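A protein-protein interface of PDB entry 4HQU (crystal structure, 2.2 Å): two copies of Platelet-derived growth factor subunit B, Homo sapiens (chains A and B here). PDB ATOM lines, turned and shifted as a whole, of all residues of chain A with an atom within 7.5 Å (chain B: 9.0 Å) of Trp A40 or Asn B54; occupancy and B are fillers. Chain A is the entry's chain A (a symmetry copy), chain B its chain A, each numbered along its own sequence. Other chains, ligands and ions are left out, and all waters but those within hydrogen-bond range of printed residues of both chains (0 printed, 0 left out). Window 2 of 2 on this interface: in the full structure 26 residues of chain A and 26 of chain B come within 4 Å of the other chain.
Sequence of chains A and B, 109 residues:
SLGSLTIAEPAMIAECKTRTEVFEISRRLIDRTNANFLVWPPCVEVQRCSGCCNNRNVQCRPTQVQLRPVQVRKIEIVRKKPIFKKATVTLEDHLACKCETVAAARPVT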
ATOM      1  N   ILE A  25     -24.806   8.951 -18.003  1.00  0.00           N
ATOM      2  CA  ILE A  25     -25.447   8.617 -19.276  1.00  0.00           C
ATOM      3  C   ILE A  25     -24.501   7.817 -20.156  1.00  0.00           C
ATOM      4  O   ILE A  25     -23.390   8.247 -20.449  1.00  0.00           O
ATOM      5  CB  ILE A  25     -25.998   9.867 -19.989  1.00  0.00           C
ATOM      6  CG1 ILE A  25     -27.336  10.253 -19.354  1.00  0.00           C
ATOM      7  CG2 ILE A  25     -26.229   9.602 -21.470  1.00  0.00           C
ATOM      8  CD1 ILE A  25     -27.673  11.708 -19.510  1.00  0.00           C
ATOM      9  N   ARG A  27     -22.920   6.429 -23.287  1.00  0.00           N
ATOM     10  CA  ARG A  27     -22.783   6.714 -24.721  1.00  0.00           C
ATOM     11  C   ARG A  27     -23.021   5.446 -25.543  1.00  0.00           C
ATOM     12  O   ARG A  27     -23.570   5.505 -26.648  1.00  0.00           O
ATOM     13  CB  ARG A  27     -21.415   7.327 -25.033  1.00  0.00           C
ATOM     14  CG  ARG A  27     -21.309   8.793 -24.641  1.00  0.00           C
ATOM     15  CD  ARG A  27     -19.890   9.333 -24.754  1.00  0.00           C
ATOM     16  NE  ARG A  27     -19.454   9.498 -26.140  1.00  0.00           N
ATOM     17  CZ  ARG A  27     -18.486   8.786 -26.713  1.00  0.00           C
ATOM     18  NH1 ARG A  27     -17.841   7.851 -26.025  1.00  0.00           N
ATOM     19  NH2 ARG A  27     -18.168   9.003 -27.984  1.00  0.00           N
ATOM     20  N   ILE A  30     -26.584   4.968 -26.444  1.00  0.00           N
ATOM     21  CA  ILE A  30     -26.920   5.963 -27.465  1.00  0.00           C
ATOM     22  C   ILE A  30     -26.494   5.486 -28.857  1.00  0.00           C
ATOM     23  O   ILE A  30     -27.295   5.523 -29.791  1.00  0.00           O
ATOM     24  CB  ILE A  30     -26.349   7.355 -27.132  1.00  0.00           C
ATOM     25  CG1 ILE A  30     -27.178   7.978 -26.002  1.00  0.00           C
ATOM     26  CG2 ILE A  30     -26.375   8.256 -28.363  1.00  0.00           C
ATOM     27  CD1 ILE A  30     -26.467   9.034 -25.194  1.00  0.00           C
ATOM     28  N   LEU A  38     -20.431  13.207 -29.336  1.00  0.00           N
ATOM     29  CA  LEU A  38     -20.421  13.701 -27.972  1.00  0.00           C
ATOM     30  C   LEU A  38     -21.855  13.839 -27.513  1.00  0.00           C
ATOM     31  O   LEU A  38     -22.750  14.036 -28.342  1.00  0.00           O
ATOM     32  CB  LEU A  38     -19.734  15.056 -27.896  1.00  0.00           C
ATOM     33  CG  LEU A  38     -18.242  15.157 -28.216  1.00  0.00           C
ATOM     34  CD1 LEU A  38     -17.844  16.617 -28.361  1.00  0.00           C
ATOM     35  CD2 LEU A  38     -17.418  14.486 -27.136  1.00  0.00           C
ATOM     36  N   VAL A  39     -22.067  13.719 -26.196  1.00  0.00           N
ATOM     37  CA  VAL A  39     -23.395  13.862 -25.610  1.00  0.00           C
ATOM     38  C   VAL A  39     -23.357  14.855 -24.452  1.00  0.00           C
ATOM     39  O   VAL A  39     -22.321  15.027 -23.802  1.00  0.00           O
ATOM     40  CB  VAL A  39     -23.966  12.490 -25.170  1.00  0.00           C
ATOM     41  CG1 VAL A  39     -25.229  12.637 -24.339  1.00  0.00           C
ATOM     42  CG2 VAL A  39     -24.253  11.621 -26.386  1.00  0.00           C
ATOM     43  N   TRP A  40     -24.489  15.510 -24.217  1.00  0.00           N
ATOM     44  CA  TRP A  40     -24.640  16.411 -23.088  1.00  0.00           C
ATOM     45  C   TRP A  40     -26.062  16.382 -22.607  1.00  0.00           C
ATOM     46  O   TRP A  40     -26.991  16.399 -23.433  1.00  0.00           O
ATOM     47  CB  TRP A  40     -24.223  17.833 -23.448  1.00  0.00           C
ATOM     48  CG  TRP A  40     -24.143  18.707 -22.220  1.00  0.00           C
ATOM     49  CD1 TRP A  40     -25.151  19.491 -21.662  1.00  0.00           C
ATOM     50  CD2 TRP A  40     -22.993  18.860 -21.319  1.00  0.00           C
ATOM     51  NE1 TRP A  40     -24.700  20.119 -20.529  1.00  0.00           N
ATOM     52  CE2 TRP A  40     -23.414  19.784 -20.272  1.00  0.00           C
ATOM     53  CE3 TRP A  40     -21.699  18.351 -21.294  1.00  0.00           C
ATOM     54  CZ2 TRP A  40     -22.571  20.156 -19.241  1.00  0.00           C
ATOM     55  CZ3 TRP A  40     -20.844  18.747 -20.256  1.00  0.00           C
ATOM     56  CH2 TRP A  40     -21.276  19.624 -19.252  1.00  0.00           C
ATOM     57  N   PRO A  41     -26.271  16.320 -21.267  1.00  0.00           N
ATOM     58  CA  PRO A  41     -25.306  16.276 -20.155  1.00  0.00           C
ATOM     59  C   PRO A  41     -24.732  14.877 -19.940  1.00  0.00           C
ATOM     60  O   PRO A  41     -25.307  13.899 -20.429  1.00  0.00           O
ATOM     61  CB  PRO A  41     -26.159  16.672 -18.951  1.00  0.00           C
ATOM     62  CG  PRO A  41     -27.515  16.143 -19.273  1.00  0.00           C
ATOM     63  CD  PRO A  41     -27.660  16.237 -20.780  1.00  0.00           C
ATOM     64  N   PRO A  42     -23.593  14.769 -19.229  1.00  0.00           N
ATOM     65  CA  PRO A  42     -23.049  13.439 -19.017  1.00  0.00           C
ATOM     66  C   PRO A  42     -23.739  12.632 -17.885  1.00  0.00           C
ATOM     67  O   PRO A  42     -23.572  11.415 -17.843  1.00  0.00           O
ATOM     68  CB  PRO A  42     -21.584  13.720 -18.664  1.00  0.00           C
ATOM     69  CG  PRO A  42     -21.628  15.060 -17.978  1.00  0.00           C
ATOM     70  CD  PRO A  42     -22.741  15.826 -18.643  1.00  0.00           C
ATOM     71  N   CYS A  43     -24.485  13.297 -16.990  1.00  0.00           N
ATOM     72  CA  CYS A  43     -25.153  12.637 -15.850  1.00  0.00           C
ATOM     73  C   CYS A  43     -26.426  13.333 -15.434  1.00  0.00           C
ATOM     74  O   CYS A  43     -26.527  14.551 -15.553  1.00  0.00           O
ATOM     75  CB  CYS A  43     -24.252  12.638 -14.622  1.00  0.00           C
ATOM     76  SG  CYS A  43     -22.563  12.116 -14.968  1.00  0.00           S
ATOM     77  N   VAL A  44     -27.366  12.557 -14.893  1.00  0.00           N
ATOM     78  CA  VAL A  44     -28.661  13.057 -14.448  1.00  0.00           C
ATOM     79  C   VAL A  44     -29.010  12.431 -13.087  1.00  0.00           C
ATOM     80  O   VAL A  44     -28.413  11.434 -12.674  1.00  0.00           O
ATOM     81  CB  VAL A  44     -29.784  12.717 -15.457  1.00  0.00           C
ATOM     82  CG1 VAL A  44     -29.593  13.480 -16.765  1.00  0.00           C
ATOM     83  CG2 VAL A  44     -29.822  11.216 -15.722  1.00  0.00           C
ATOM     84  N   GLN A  71     -34.325  13.857 -23.025  1.00  0.00           N
ATOM     85  CA  GLN A  71     -33.751  14.226 -24.308  1.00  0.00           C
ATOM     86  C   GLN A  71     -32.350  14.733 -24.063  1.00  0.00           C
ATOM     87  O   GLN A  71     -32.149  15.676 -23.303  1.00  0.00           O
ATOM     88  CB  GLN A  71     -34.597  15.328 -24.950  1.00  0.00           C
ATOM     89  CG  GLN A  71     -34.524  15.404 -26.466  1.00  0.00           C
ATOM     90  CD  GLN A  71     -35.583  16.331 -27.057  1.00  0.00           C
ATOM     91  OE1 GLN A  71     -35.645  17.523 -26.727  1.00  0.00           O
ATOM     92  NE2 GLN A  71     -36.426  15.785 -27.938  1.00  0.00           N
ATOM     93  N   VAL A  72     -31.373  14.099 -24.685  1.00  0.00           N
ATOM     94  CA  VAL A  72     -30.005  14.568 -24.551  1.00  0.00           C
ATOM     95  C   VAL A  72     -29.522  15.232 -25.832  1.00  0.00           C
ATOM     96  O   VAL A  72     -30.064  14.991 -26.914  1.00  0.00           O
ATOM     97  CB  VAL A  72     -29.039  13.451 -24.107  1.00  0.00           C
ATOM     98  CG1 VAL A  72     -29.484  12.888 -22.763  1.00  0.00           C
ATOM     99  CG2 VAL A  72     -28.955  12.355 -25.150  1.00  0.00           C
ATOM    100  N   ARG A  73     -28.519  16.091 -25.691  1.00  0.00           N
ATOM    101  CA  ARG A  73     -27.886  16.739 -26.824  1.00  0.00           C
ATOM    102  C   ARG A  73     -26.768  15.861 -27.354  1.00  0.00           C
ATOM    103  O   ARG A  73     -25.967  15.332 -26.575  1.00  0.00           O
ATOM    104  CB  ARG A  73     -27.350  18.098 -26.409  1.00  0.00           C
ATOM    105  CG  ARG A  73     -28.435  19.146 -26.403  1.00  0.00           C
ATOM    106  CD  ARG A  73     -28.314  20.103 -25.237  1.00  0.00           C
ATOM    107  NE  ARG A  73     -29.055  21.318 -25.554  1.00  0.00           N
ATOM    108  CZ  ARG A  73     -28.517  22.527 -25.661  1.00  0.00           C
ATOM    109  NH1 ARG A  73     -29.290  23.550 -25.982  1.00  0.00           N
ATOM    110  NH2 ARG A  73     -27.220  22.718 -25.426  1.00  0.00           N
ATOM    111  N   LYS A  74     -26.726  15.712 -28.678  1.00  0.00           N
ATOM    112  CA  LYS A  74     -25.720  14.894 -29.345  1.00  0.00           C
ATOM    113  C   LYS A  74     -25.061  15.695 -30.458  1.00  0.00           C
ATOM    114  O   LYS A  74     -25.738  16.335 -31.266  1.00  0.00           O
ATOM    115  CB  LYS A  74     -26.359  13.627 -29.927  1.00  0.00           C
ATOM    116  CG  LYS A  74     -25.371  12.647 -30.551  1.00  0.00           C
ATOM    117  CD  LYS A  74     -26.086  11.525 -31.297  1.00  0.00           C
ATOM    118  CE  LYS A  74     -25.074  10.532 -31.861  1.00  0.00           C
ATOM    119  NZ  LYS A  74     -25.704   9.497 -32.726  1.00  0.00           N
ATOM    120  N   ILE A  75     -23.735  15.666 -30.485  1.00  0.00           N
ATOM    121  CA  ILE A  75     -22.986  16.212 -31.600  1.00  0.00           C
ATOM    122  C   ILE A  75     -22.294  15.054 -32.312  1.00  0.00           C
ATOM    123  O   ILE A  75     -21.509  14.328 -31.707  1.00  0.00           O
ATOM    124  CB  ILE A  75     -21.908  17.203 -31.138  1.00  0.00           C
ATOM    125  CG1 ILE A  75     -22.547  18.466 -30.554  1.00  0.00           C
ATOM    126  CG2 ILE A  75     -20.961  17.525 -32.293  1.00  0.00           C
ATOM    127  CD1 ILE A  75     -21.563  19.399 -29.880  1.00  0.00           C
ATOM    128  N   ALA A  87     -30.915  12.850 -28.937  1.00  0.00           N
ATOM    129  CA  ALA A  87     -31.137  11.439 -28.631  1.00  0.00           C
ATOM    130  C   ALA A  87     -32.018  11.339 -27.402  1.00  0.00           C
ATOM    131  O   ALA A  87     -32.064  12.249 -26.581  1.00  0.00           O
ATOM    132  CB  ALA A  87     -29.819  10.722 -28.405  1.00  0.00           C
ATOM    133  N   PRO B  10     -36.172  17.717 -21.349  1.00  0.00           N
ATOM    134  CA  PRO B  10     -34.726  17.852 -21.535  1.00  0.00           C
ATOM    135  C   PRO B  10     -33.955  17.280 -20.344  1.00  0.00           C
ATOM    136  O   PRO B  10     -34.296  17.559 -19.196  1.00  0.00           O
ATOM    137  CB  PRO B  10     -34.510  19.365 -21.608  1.00  0.00           C
ATOM    138  CG  PRO B  10     -35.850  19.951 -21.887  1.00  0.00           C
ATOM    139  CD  PRO B  10     -36.844  19.024 -21.265  1.00  0.00           C
ATOM    140  N   ALA B  11     -32.927  16.486 -20.627  1.00  0.00           N
ATOM    141  CA  ALA B  11     -32.042  15.982 -19.587  1.00  0.00           C
ATOM    142  C   ALA B  11     -31.378  17.158 -18.873  1.00  0.00           C
ATOM    143  O   ALA B  11     -30.965  18.113 -19.516  1.00  0.00           O
ATOM    144  CB  ALA B  11     -31.000  15.066 -20.198  1.00  0.00           C
ATOM    145  N   MET B  12     -31.305  17.091 -17.546  1.00  0.00           N
ATOM    146  CA  MET B  12     -30.685  18.136 -16.725  1.00  0.00           C
ATOM    147  C   MET B  12     -29.450  17.562 -16.032  1.00  0.00           C
ATOM    148  O   MET B  12     -29.505  16.478 -15.450  1.00  0.00           O
ATOM    149  CB  MET B  12     -31.670  18.637 -15.657  1.00  0.00           C
ATOM    150  CG  MET B  12     -32.958  19.258 -16.191  1.00  0.00           C
ATOM    151  SD  MET B  12     -32.657  20.845 -17.000  1.00  0.00           S
ATOM    152  CE  MET B  12     -32.074  21.831 -15.612  1.00  0.00           C
ATOM    153  N   ILE B  13     -28.339  18.287 -16.075  1.00  0.00           N
ATOM    154  CA  ILE B  13     -27.122  17.778 -15.479  1.00  0.00           C
ATOM    155  C   ILE B  13     -27.263  17.578 -13.955  1.00  0.00           C
ATOM    156  O   ILE B  13     -27.869  18.390 -13.262  1.00  0.00           O
ATOM    157  CB  ILE B  13     -25.887  18.643 -15.822  1.00  0.00           C
ATOM    158  CG1 ILE B  13     -24.615  17.901 -15.407  1.00  0.00           C
ATOM    159  CG2 ILE B  13     -26.001  20.038 -15.202  1.00  0.00           C
ATOM    160  CD1 ILE B  13     -23.329  18.424 -15.999  1.00  0.00           C
ATOM    161  N   ALA B  14     -26.732  16.472 -13.454  1.00  0.00           N
ATOM    162  CA  ALA B  14     -26.625  16.274 -12.015  1.00  0.00           C
ATOM    163  C   ALA B  14     -25.406  17.067 -11.588  1.00  0.00           C
ATOM    164  O   ALA B  14     -24.257  16.635 -11.793  1.00  0.00           O
ATOM    165  CB  ALA B  14     -26.467  14.799 -11.689  1.00  0.00           C
ATOM    166  N   GLU B  15     -25.672  18.247 -11.026  1.00  0.00           N
ATOM    167  CA  GLU B  15     -24.641  19.189 -10.598  1.00  0.00           C
ATOM    168  C   GLU B  15     -23.802  18.591  -9.475  1.00  0.00           C
ATOM    169  O   GLU B  15     -24.263  17.686  -8.747  1.00  0.00           O
ATOM    170  CB  GLU B  15     -25.277  20.520 -10.142  1.00  0.00           C
ATOM    171  N   CYS B  16     -22.564  19.068  -9.377  1.00  0.00           N
ATOM    172  CA  CYS B  16     -21.681  18.732  -8.282  1.00  0.00           C
ATOM    173  C   CYS B  16     -22.222  19.443  -7.062  1.00  0.00           C
ATOM    174  O   CYS B  16     -22.150  20.668  -6.985  1.00  0.00           O
ATOM    175  CB  CYS B  16     -20.257  19.192  -8.576  1.00  0.00           C
ATOM    176  SG  CYS B  16     -19.133  19.098  -7.159  1.00  0.00           S
ATOM    177  N   GLY B  51     -21.999  14.071  -8.240  1.00  0.00           N
ATOM    178  CA  GLY B  51     -22.438  14.774  -9.433  1.00  0.00           C
ATOM    179  C   GLY B  51     -21.283  14.888 -10.398  1.00  0.00           C
ATOM    180  O   GLY B  51     -20.168  14.438 -10.110  1.00  0.00           O
ATOM    181  N   CYS B  52     -21.537  15.500 -11.546  1.00  0.00           N
ATOM    182  CA  CYS B  52     -20.534  15.539 -12.603  1.00  0.00           C
ATOM    183  C   CYS B  52     -20.129  16.941 -12.987  1.00  0.00           C
ATOM    184  O   CYS B  52     -20.971  17.819 -13.134  1.00  0.00           O
ATOM    185  CB  CYS B  52     -21.040  14.782 -13.819  1.00  0.00           C
ATOM    186  SG  CYS B  52     -21.418  13.091 -13.337  1.00  0.00           S
ATOM    187  N   CYS B  53     -18.827  17.126 -13.146  1.00  0.00           N
ATOM    188  CA  CYS B  53     -18.263  18.390 -13.602  1.00  0.00           C
ATOM    189  C   CYS B  53     -18.202  18.446 -15.149  1.00  0.00           C
ATOM    190  O   CYS B  53     -18.588  17.482 -15.823  1.00  0.00           O
ATOM    191  CB  CYS B  53     -16.889  18.587 -12.963  1.00  0.00           C
ATOM    192  SG  CYS B  53     -16.905  18.539 -11.145  1.00  0.00           S
ATOM    193  N   ASN B  54     -17.732  19.570 -15.694  1.00  0.00           N
ATOM    194  CA  ASN B  54     -17.706  19.839 -17.145  1.00  0.00           C
ATOM    195  C   ASN B  54     -16.914  18.860 -17.980  1.00  0.00           C
ATOM    196  O   ASN B  54     -17.275  18.572 -19.121  1.00  0.00           O
ATOM    197  CB  ASN B  54     -17.110  21.220 -17.408  1.00  0.00           C
ATOM    198  CG  ASN B  54     -18.145  22.312 -17.376  1.00  0.00           C
ATOM    199  OD1 ASN B  54     -17.805  23.488 -17.242  1.00  0.00           O
ATOM    200  ND2 ASN B  54     -19.423  21.933 -17.496  1.00  0.00           N
ATOM    201  N   ASN B  55     -15.809  18.390 -17.415  1.00  0.00           N
ATOM    202  CA  ASN B  55     -14.861  17.545 -18.131  1.00  0.00           C
ATOM    203  C   ASN B  55     -14.093  16.657 -17.155  1.00  0.00           C
ATOM    204  O   ASN B  55     -14.151  16.867 -15.942  1.00  0.00           O
ATOM    205  CB  ASN B  55     -13.890  18.393 -18.971  1.00  0.00           C
ATOM    206  CG  ASN B  55     -13.034  19.315 -18.122  1.00  0.00           C
ATOM    207  OD1 ASN B  55     -11.878  19.005 -17.833  1.00  0.00           O
ATOM    208  ND2 ASN B  55     -13.602  20.445 -17.705  1.00  0.00           N
ATOM    209  N   ARG B  56     -13.365  15.684 -17.697  1.00  0.00           N
ATOM    210  CA  ARG B  56     -12.668  14.686 -16.891  1.00  0.00           C
ATOM    211  C   ARG B  56     -11.294  15.121 -16.377  1.00  0.00           C
ATOM    212  O   ARG B  56     -10.548  14.308 -15.832  1.00  0.00           O
ATOM    213  CB  ARG B  56     -12.591  13.369 -17.653  1.00  0.00           C
ATOM    214  CG  ARG B  56     -13.951  12.710 -17.771  1.00  0.00           C
ATOM    215  CD  ARG B  56     -13.878  11.419 -18.556  1.00  0.00           C
ATOM    216  NE  ARG B  56     -14.890  10.484 -18.086  1.00  0.00           N
ATOM    217  CZ  ARG B  56     -16.100  10.348 -18.617  1.00  0.00           C
ATOM    218  NH1 ARG B  56     -16.469  11.083 -19.659  1.00  0.00           N
ATOM    219  NH2 ARG B  56     -16.939   9.465 -18.103  1.00  0.00           N
ATOM    220  N   ASN B  57     -10.961  16.397 -16.544  1.00  0.00           N
ATOM    221  CA  ASN B  57      -9.769  16.948 -15.910  1.00  0.00           C
ATOM    222  C   ASN B  57     -10.075  17.422 -14.485  1.00  0.00           C
ATOM    223  O   ASN B  57      -9.158  17.689 -13.700  1.00  0.00           O
ATOM    224  CB  ASN B  57      -9.153  18.069 -16.759  1.00  0.00           C
ATOM    225  N   VAL B  58     -11.366  17.519 -14.158  1.00  0.00           N
ATOM    226  CA  VAL B  58     -11.811  17.895 -12.809  1.00  0.00           C
ATOM    227  C   VAL B  58     -12.769  16.871 -12.197  1.00  0.00           C
ATOM    228  O   VAL B  58     -13.468  16.153 -12.917  1.00  0.00           O
ATOM    229  CB  VAL B  58     -12.478  19.297 -12.761  1.00  0.00           C
ATOM    230  CG1 VAL B  58     -11.442  20.402 -12.936  1.00  0.00           C
ATOM    231  CG2 VAL B  58     -13.592  19.415 -13.796  1.00  0.00           C
ATOM    232  N   GLN B  59     -12.796  16.822 -10.865  1.00  0.00           N
ATOM    233  CA  GLN B  59     -13.708  15.951 -10.124  1.00  0.00           C
ATOM    234  C   GLN B  59     -14.410  16.681  -8.982  1.00  0.00           C
ATOM    235  O   GLN B  59     -13.868  17.626  -8.406  1.00  0.00           O
ATOM    236  CB  GLN B  59     -12.963  14.729  -9.590  1.00  0.00           C
ATOM    237  CG  GLN B  59     -12.788  13.621 -10.617  1.00  0.00           C
ATOM    238  CD  GLN B  59     -11.880  12.511 -10.121  1.00  0.00           C
ATOM    239  OE1 GLN B  59     -10.743  12.761  -9.719  1.00  0.00           O
ATOM    240  NE2 GLN B  59     -12.378  11.275 -10.146  1.00  0.00           N
ATOM    241  N   CYS B  60     -15.626  16.240  -8.678  1.00  0.00           N
ATOM    242  CA  CYS B  60     -16.440  16.805  -7.615  1.00  0.00           C
ATOM    243  C   CYS B  60     -15.890  16.394  -6.239  1.00  0.00           C
ATOM    244  O   CYS B  60     -15.858  15.209  -5.912  1.00  0.00           O
ATOM    245  CB  CYS B  60     -17.876  16.323  -7.786  1.00  0.00           C
ATOM    246  SG  CYS B  60     -19.055  17.096  -6.688  1.00  0.00           S
ATOM    247  N   CYS B  99     -15.858  21.571  -8.211  1.00  0.00           N
ATOM    248  CA  CYS B  99     -15.108  20.842  -9.213  1.00  0.00           C
ATOM    249  C   CYS B  99     -13.639  21.243  -9.119  1.00  0.00           C
ATOM    250  O   CYS B  99     -13.306  22.422  -9.136  1.00  0.00           O
ATOM    251  CB  CYS B  99     -15.688  21.103 -10.604  1.00  0.00           C
ATOM    252  SG  CYS B  99     -17.391  20.512 -10.774  1.00  0.00           S
ATOM    253  N   GLU B 100     -12.773  20.242  -9.024  1.00  0.00           N
ATOM    254  CA  GLU B 100     -11.395  20.418  -8.601  1.00  0.00           C
ATOM    255  C   GLU B 100     -10.496  19.609  -9.515  1.00  0.00           C
ATOM    256  O   GLU B 100     -10.869  18.521  -9.938  1.00  0.00           O
ATOM    257  CB  GLU B 100     -11.264  19.890  -7.179  1.00  0.00           C
ATOM    258  CG  GLU B 100     -10.119  20.454  -6.369  1.00  0.00           C
ATOM    259  CD  GLU B 100     -10.383  20.301  -4.887  1.00  0.00           C
ATOM    260  OE1 GLU B 100     -11.094  21.161  -4.325  1.00  0.00           O
ATOM    261  OE2 GLU B 100      -9.896  19.317  -4.289  1.00  0.00           O
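N of Ile A25 is in hydrogen-bond range of O of Pro A42 (2.8 Å). O of Ala B14 is in hydrogen-bond range of N of Cys B52, 3.0 Å away. The side-chain sulfur (SG) of Cys B16 forms a disulfide with the side-chain sulfur (SG) of Cys B60 (2.1 Å). The backbone carbonyl oxygen (O) of Trp A40 is in hydrogen-bond range of the backbone NH (N) of Arg A73. The backbone carbonyl oxygen of Ala A87 lies within hydrogen-bond range of the backbone NH of Val A72, at 2.7 Å. The side-chain sulfur (SG) of Cys B53 forms a disulfide with the side-chain sulfur (SG) of Cys B99, at 2.1 Å.
The backbone carbonyl oxygen (O) of Gln A71 lies within hydrogen-bond range of the backbone NH (N) of Ala B11, 2.9 Å away. The side-chain sulfur (SG) of Cys A43 is disulfide-bonded to the side-chain sulfur (SG) of Cys B52, at 2.2 Å. N of Ala B14 sits at hydrogen-bond distance from O of Cys A43.
Of the printed residues of chain B, Trp A40 touches Ile B13 (3.8 Å) and Asn B54 (3.4 Å). Of chain A, only Trp A40 (3.4 Å) comes within 4 Å of Asn B54. Of chain B, only Ala B11 and Ile B13 come within 4 Å of Pro A41. Of the printed residues of chain A, Met B12 touches Cys A43 (3.5 Å) and Val A44 (3.3 Å). Of the printed residues of chain A, Pro B10 touches Gln A71. Of the printed residues of chain A, Cys B52 touches Cys A43 (2.2 Å). Of the printed residues of chain B, Val A44 touches Met B12 (3.3 Å) and Ala B14 (3.7 Å). Of the printed residues of chain A, Ala B14 touches Cys A43 (2.9 Å) and Val A44 (3.7 Å). The nearest residue of chain B that does not touch Trp A40 is Cys B53 (4.9 Å). The nearest printed residue of chain B that does not touch Cys A43 is Gly B51 (5.5 Å).
Of the 19 printed residues of chain B, 7 touch a printed residue of chain A. Printed residues of chain B that touch a printed residue of chain A: Pro B10, Ala B11, Met B12, Ile B13, Ala B14, Cys B52 and Asn B54. Hydrophobic or aromatic side chains of chain B within 4 Å of the printed part of chain A: Ala B11, Ile B13 and Ala B14. Hydrophobic or aromatic side chains of chain A that line the printed part of chain B: Trp A40, Pro A41, Pro A42, Val A44 and Val A72. Along chain A the printed residues that touch a printed residue of chain B span positions 40 to 72. Among the printed residues, 14 pairs touch across the chains. Among the printed residues, no Asp or Glu carboxylate lies within 4 Å of a Lys or Arg side-chain nitrogen of the other chain.
Ile B13 touches Trp A40 (CD1 to CZ2, 3.8 Å). Trp A40 touches Asn B54 (CH2 to ND2, 3.4 Å). CB of Ala B11 touches CD of Pro A41, 3.6 Å away. CB of Pro A41 touches CB of Ile B13, at 3.7 Å. Ile B13 touches Pro A42 (CD1 to CD, 3.8 Å). Cys A43 touches Met B12. Val A44 touches Met B12. Ala B14 touches Val A44. Pro B10 touches Gln A71. Val A72 touches Ala B11 (CG1 to CB, 3.7 Å).
No position is printed for both chains.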
